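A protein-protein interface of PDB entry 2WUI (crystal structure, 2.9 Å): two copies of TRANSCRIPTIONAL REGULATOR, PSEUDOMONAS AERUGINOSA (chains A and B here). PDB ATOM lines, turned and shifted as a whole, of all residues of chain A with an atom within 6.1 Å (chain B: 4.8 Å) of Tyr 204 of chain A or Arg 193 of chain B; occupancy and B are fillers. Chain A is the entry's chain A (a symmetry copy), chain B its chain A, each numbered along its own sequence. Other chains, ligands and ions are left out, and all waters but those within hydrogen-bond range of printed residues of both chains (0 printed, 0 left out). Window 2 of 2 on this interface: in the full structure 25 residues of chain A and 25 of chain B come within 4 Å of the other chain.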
ATOM      1  N   LEU A 158       5.133  -0.845 -23.426  1.00  0.00           N
ATOM      2  CA  LEU A 158       4.849   0.582 -23.408  1.00  0.00           C
ATOM      3  C   LEU A 158       5.111   1.197 -24.777  1.00  0.00           C
ATOM      4  O   LEU A 158       4.393   2.096 -25.201  1.00  0.00           O
ATOM      5  CB  LEU A 158       5.683   1.282 -22.356  1.00  0.00           C
ATOM      6  CG  LEU A 158       4.920   2.378 -21.620  1.00  0.00           C
ATOM      7  CD1 LEU A 158       5.831   3.551 -21.368  1.00  0.00           C
ATOM      8  CD2 LEU A 158       3.748   2.817 -22.433  1.00  0.00           C
ATOM      9  N   SER A 202      14.872   7.592 -26.734  1.00  0.00           N
ATOM     10  CA  SER A 202      14.216   8.256 -25.630  1.00  0.00           C
ATOM     11  C   SER A 202      14.221   7.390 -24.409  1.00  0.00           C
ATOM     12  O   SER A 202      13.619   6.311 -24.413  1.00  0.00           O
ATOM     13  CB  SER A 202      12.799   8.694 -25.975  1.00  0.00           C
ATOM     14  OG  SER A 202      12.467   9.861 -25.245  1.00  0.00           O
ATOM     15  N   PRO A 203      14.939   7.862 -23.372  1.00  0.00           N
ATOM     16  CA  PRO A 203      15.107   7.360 -22.008  1.00  0.00           C
ATOM     17  C   PRO A 203      13.817   6.749 -21.487  1.00  0.00           C
ATOM     18  O   PRO A 203      13.795   5.577 -21.088  1.00  0.00           O
ATOM     19  CB  PRO A 203      15.387   8.638 -21.215  1.00  0.00           C
ATOM     20  CG  PRO A 203      15.985   9.602 -22.189  1.00  0.00           C
ATOM     21  CD  PRO A 203      15.728   9.088 -23.591  1.00  0.00           C
ATOM     22  N   TYR A 204      12.749   7.544 -21.497  1.00  0.00           N
ATOM     23  CA  TYR A 204      11.515   7.198 -20.798  1.00  0.00           C
ATOM     24  C   TYR A 204      10.805   5.965 -21.347  1.00  0.00           C
ATOM     25  O   TYR A 204       9.818   5.514 -20.779  1.00  0.00           O
ATOM     26  CB  TYR A 204      10.567   8.389 -20.799  1.00  0.00           C
ATOM     27  CG  TYR A 204      11.211   9.683 -20.332  1.00  0.00           C
ATOM     28  CD1 TYR A 204      11.238  10.026 -18.980  1.00  0.00           C
ATOM     29  CD2 TYR A 204      11.790  10.559 -21.244  1.00  0.00           C
ATOM     30  CE1 TYR A 204      11.822  11.211 -18.549  1.00  0.00           C
ATOM     31  CE2 TYR A 204      12.377  11.747 -20.822  1.00  0.00           C
ATOM     32  CZ  TYR A 204      12.384  12.065 -19.476  1.00  0.00           C
ATOM     33  OH  TYR A 204      12.963  13.237 -19.053  1.00  0.00           O
ATOM     34  N   LEU A 205      11.307   5.410 -22.441  1.00  0.00           N
ATOM     35  CA  LEU A 205      10.712   4.205 -23.013  1.00  0.00           C
ATOM     36  C   LEU A 205      11.512   2.932 -22.728  1.00  0.00           C
ATOM     37  O   LEU A 205      11.053   1.835 -23.052  1.00  0.00           O
ATOM     38  CB  LEU A 205      10.469   4.358 -24.524  1.00  0.00           C
ATOM     39  CG  LEU A 205       9.060   4.759 -25.013  1.00  0.00           C
ATOM     40  CD1 LEU A 205       8.225   5.478 -23.943  1.00  0.00           C
ATOM     41  CD2 LEU A 205       9.109   5.576 -26.315  1.00  0.00           C
ATOM     42  N   LEU A 206      12.701   3.066 -22.140  1.00  0.00           N
ATOM     43  CA  LEU A 206      13.413   1.889 -21.657  1.00  0.00           C
ATOM     44  C   LEU A 206      12.740   1.471 -20.376  1.00  0.00           C
ATOM     45  O   LEU A 206      12.002   2.266 -19.795  1.00  0.00           O
ATOM     46  CB  LEU A 206      14.873   2.195 -21.339  1.00  0.00           C
ATOM     47  CG  LEU A 206      15.917   2.384 -22.437  1.00  0.00           C
ATOM     48  CD1 LEU A 206      15.576   1.584 -23.697  1.00  0.00           C
ATOM     49  CD2 LEU A 206      16.065   3.857 -22.753  1.00  0.00           C
ATOM     50  N   ASP B  83       7.235  22.236 -18.950  1.00  0.00           N
ATOM     51  CA  ASP B  83       6.868  21.745 -17.628  1.00  0.00           C
ATOM     52  C   ASP B  83       5.435  22.148 -17.366  1.00  0.00           C
ATOM     53  O   ASP B  83       4.671  21.383 -16.784  1.00  0.00           O
ATOM     54  CB  ASP B  83       7.799  22.267 -16.529  1.00  0.00           C
ATOM     55  CG  ASP B  83       8.981  21.317 -16.245  1.00  0.00           C
ATOM     56  OD1 ASP B  83       9.604  21.437 -15.155  1.00  0.00           O
ATOM     57  OD2 ASP B  83       9.282  20.449 -17.101  1.00  0.00           O
ATOM     58  N   LEU B  86       3.148  19.904 -19.923  1.00  0.00           N
ATOM     59  CA  LEU B  86       2.931  18.570 -19.375  1.00  0.00           C
ATOM     60  C   LEU B  86       2.027  18.564 -18.135  1.00  0.00           C
ATOM     61  O   LEU B  86       1.064  17.798 -18.066  1.00  0.00           O
ATOM     62  CB  LEU B  86       4.269  17.912 -19.041  1.00  0.00           C
ATOM     63  CG  LEU B  86       4.331  16.389 -18.932  1.00  0.00           C
ATOM     64  CD1 LEU B  86       5.590  15.994 -18.171  1.00  0.00           C
ATOM     65  CD2 LEU B  86       3.117  15.848 -18.240  1.00  0.00           C
ATOM     66  N   GLU B 189       2.755   9.411 -18.330  1.00  0.00           N
ATOM     67  CA  GLU B 189       3.722  10.495 -18.171  1.00  0.00           C
ATOM     68  C   GLU B 189       4.989  10.171 -18.942  1.00  0.00           C
ATOM     69  O   GLU B 189       5.534  11.025 -19.640  1.00  0.00           O
ATOM     70  CB  GLU B 189       4.027  10.723 -16.704  1.00  0.00           C
ATOM     71  CG  GLU B 189       4.993  11.852 -16.418  1.00  0.00           C
ATOM     72  CD  GLU B 189       5.605  11.740 -15.020  1.00  0.00           C
ATOM     73  OE1 GLU B 189       4.847  11.747 -14.018  1.00  0.00           O
ATOM     74  OE2 GLU B 189       6.849  11.621 -14.924  1.00  0.00           O
ATOM     75  N   ARG B 190       5.442   8.926 -18.855  1.00  0.00           N
ATOM     76  CA  ARG B 190       6.579   8.511 -19.655  1.00  0.00           C
ATOM     77  C   ARG B 190       6.283   8.776 -21.127  1.00  0.00           C
ATOM     78  O   ARG B 190       7.071   9.408 -21.829  1.00  0.00           O
ATOM     79  CB  ARG B 190       6.912   7.035 -19.418  1.00  0.00           C
ATOM     80  CG  ARG B 190       7.493   6.743 -18.032  1.00  0.00           C
ATOM     81  CD  ARG B 190       8.518   5.612 -18.103  1.00  0.00           C
ATOM     82  NE  ARG B 190       7.945   4.277 -17.916  1.00  0.00           N
ATOM     83  CZ  ARG B 190       8.492   3.166 -18.407  1.00  0.00           C
ATOM     84  NH1 ARG B 190       9.592   3.246 -19.140  1.00  0.00           N
ATOM     85  NH2 ARG B 190       7.942   1.979 -18.191  1.00  0.00           N
ATOM     86  N   MET B 191       5.136   8.321 -21.602  1.00  0.00           N
ATOM     87  CA  MET B 191       4.827   8.517 -23.011  1.00  0.00           C
ATOM     88  C   MET B 191       4.835   9.996 -23.358  1.00  0.00           C
ATOM     89  O   MET B 191       5.423  10.397 -24.371  1.00  0.00           O
ATOM     90  CB  MET B 191       3.506   7.863 -23.385  1.00  0.00           C
ATOM     91  CG  MET B 191       3.368   6.480 -22.791  1.00  0.00           C
ATOM     92  SD  MET B 191       2.020   5.560 -23.543  1.00  0.00           S
ATOM     93  CE  MET B 191       2.923   4.680 -24.804  1.00  0.00           C
ATOM     94  N   PHE B 192       4.209  10.812 -22.518  1.00  0.00           N
ATOM     95  CA  PHE B 192       4.174  12.235 -22.810  1.00  0.00           C
ATOM     96  C   PHE B 192       5.568  12.820 -22.889  1.00  0.00           C
ATOM     97  O   PHE B 192       5.878  13.559 -23.820  1.00  0.00           O
ATOM     98  CB  PHE B 192       3.357  12.980 -21.772  1.00  0.00           C
ATOM     99  CG  PHE B 192       1.877  12.822 -21.946  1.00  0.00           C
ATOM    100  CD1 PHE B 192       1.242  13.370 -23.035  1.00  0.00           C
ATOM    101  CD2 PHE B 192       1.124  12.136 -21.018  1.00  0.00           C
ATOM    102  CE1 PHE B 192      -0.110  13.233 -23.201  1.00  0.00           C
ATOM    103  CE2 PHE B 192      -0.242  11.998 -21.178  1.00  0.00           C
ATOM    104  CZ  PHE B 192      -0.858  12.551 -22.273  1.00  0.00           C
ATOM    105  N   ARG B 193       6.408  12.493 -21.906  1.00  0.00           N
ATOM    106  CA  ARG B 193       7.776  13.009 -21.868  1.00  0.00           C
ATOM    107  C   ARG B 193       8.482  12.615 -23.139  1.00  0.00           C
ATOM    108  O   ARG B 193       9.068  13.458 -23.818  1.00  0.00           O
ATOM    109  CB  ARG B 193       8.529  12.455 -20.671  1.00  0.00           C
ATOM    110  CG  ARG B 193       8.016  13.005 -19.351  1.00  0.00           C
ATOM    111  CD  ARG B 193       9.089  12.927 -18.285  1.00  0.00           C
ATOM    112  NE  ARG B 193       9.301  14.231 -17.668  1.00  0.00           N
ATOM    113  CZ  ARG B 193       8.649  14.648 -16.596  1.00  0.00           C
ATOM    114  NH1 ARG B 193       8.883  15.855 -16.098  1.00  0.00           N
ATOM    115  NH2 ARG B 193       7.766  13.849 -16.021  1.00  0.00           N
ATOM    116  N   ALA B 194       8.388  11.330 -23.471  1.00  0.00           N
ATOM    117  CA  ALA B 194       8.978  10.799 -24.697  1.00  0.00           C
ATOM    118  C   ALA B 194       8.388  11.479 -25.929  1.00  0.00           C
ATOM    119  O   ALA B 194       9.004  11.532 -26.985  1.00  0.00           O
ATOM    120  CB  ALA B 194       8.778   9.295 -24.774  1.00  0.00           C
ATOM    121  N   GLY B 195       7.183  12.001 -25.797  1.00  0.00           N
ATOM    122  CA  GLY B 195       6.578  12.700 -26.910  1.00  0.00           C
ATOM    123  C   GLY B 195       7.267  14.036 -27.037  1.00  0.00           C
ATOM    124  O   GLY B 195       7.576  14.488 -28.143  1.00  0.00           O
ATOM    125  N   LEU B 196       7.520  14.661 -25.891  1.00  0.00           N
ATOM    126  CA  LEU B 196       8.155  15.970 -25.847  1.00  0.00           C
ATOM    127  C   LEU B 196       9.617  15.933 -26.317  1.00  0.00           C
ATOM    128  O   LEU B 196      10.100  16.871 -26.957  1.00  0.00           O
ATOM    129  CB  LEU B 196       8.047  16.527 -24.442  1.00  0.00           C
ATOM    130  CG  LEU B 196       6.580  16.691 -24.056  1.00  0.00           C
ATOM    131  CD1 LEU B 196       6.395  16.709 -22.552  1.00  0.00           C
ATOM    132  CD2 LEU B 196       6.035  17.970 -24.689  1.00  0.00           C
ATOM    133  N   ASP B 197      10.327  14.851 -26.024  1.00  0.00           N
ATOM    134  CA  ASP B 197      11.688  14.735 -26.537  1.00  0.00           C
ATOM    135  C   ASP B 197      11.674  14.824 -28.050  1.00  0.00           C
ATOM    136  O   ASP B 197      12.502  15.518 -28.641  1.00  0.00           O
ATOM    137  CB  ASP B 197      12.351  13.420 -26.114  1.00  0.00           C
ATOM    138  CG  ASP B 197      12.854  13.451 -24.677  1.00  0.00           C
ATOM    139  OD1 ASP B 197      12.077  13.870 -23.785  1.00  0.00           O
ATOM    140  OD2 ASP B 197      14.023  13.055 -24.439  1.00  0.00           O
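The side-chain carboxylate (OE2) of Glu 189 of chain B is in salt-bridge range of the guanidinium group (NH2) of Arg 193 of chain B, at 2.6 Å.
The guanidinium group (NH1) of Arg 190 of chain B sits at hydrogen-bond distance from the backbone carbonyl oxygen (O) of Leu 206 of chain A, 2.7 Å away. The guanidinium group (NH1) of Arg 190 of chain B is in hydrogen-bond range of the backbone carbonyl oxygen (O) of Tyr 204 of chain A (2.8 Å).
Hydrophobic or aromatic side chains of chain A that line the printed part of chain B: Leu 158, Tyr 204 and Leu 205.
No position is printed for both chains.
CZ of Arg 190 of chain B touches CD1 of Leu 158 of chain A, at 3.9996 Å. Leu 158 of chain A touches Met 191 of chain B (O to CE, 3.0 Å). Ser 202 of chain A touches Ala 194 of chain B (OG to CA, 3.7 Å). Asp 197 of chain B touches Ser 202 of chain A (OD2 to OG, 3.6 Å). Arg 193 of chain B touches Tyr 204 of chain A (CD to CE1, 3.2 Å). CE2 of Tyr 204 of chain A touches OD1 of Asp 197 of chain B, at 3.7 Å. CB of Ala 194 of chain B touches CD1 of Leu 205 of chain A, 3.9 Å away.
Of the printed residues of chain B, Tyr 204 of chain A touches Arg 190, Arg 193 and Asp 197. Arg 193 of chain B touches one residue of chain A. Of the printed residues of chain B, Ser 202 of chain A touches Ala 194 and Asp 197. Of the printed residues of chain A, Ala 194 of chain B touches Ser 202 and Leu 205. Of the printed residues of chain B, Leu 205 of chain A touches Ala 194. Of the printed residues of chain A, Asp 197 of chain B touches Ser 202 and Tyr 204. Gly 195 of chain B touches none of the printed residues of chain A. The nearest printed residue of chain B that does not touch Leu 205 of chain A is Arg 190 of chain B (4.1 Å).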
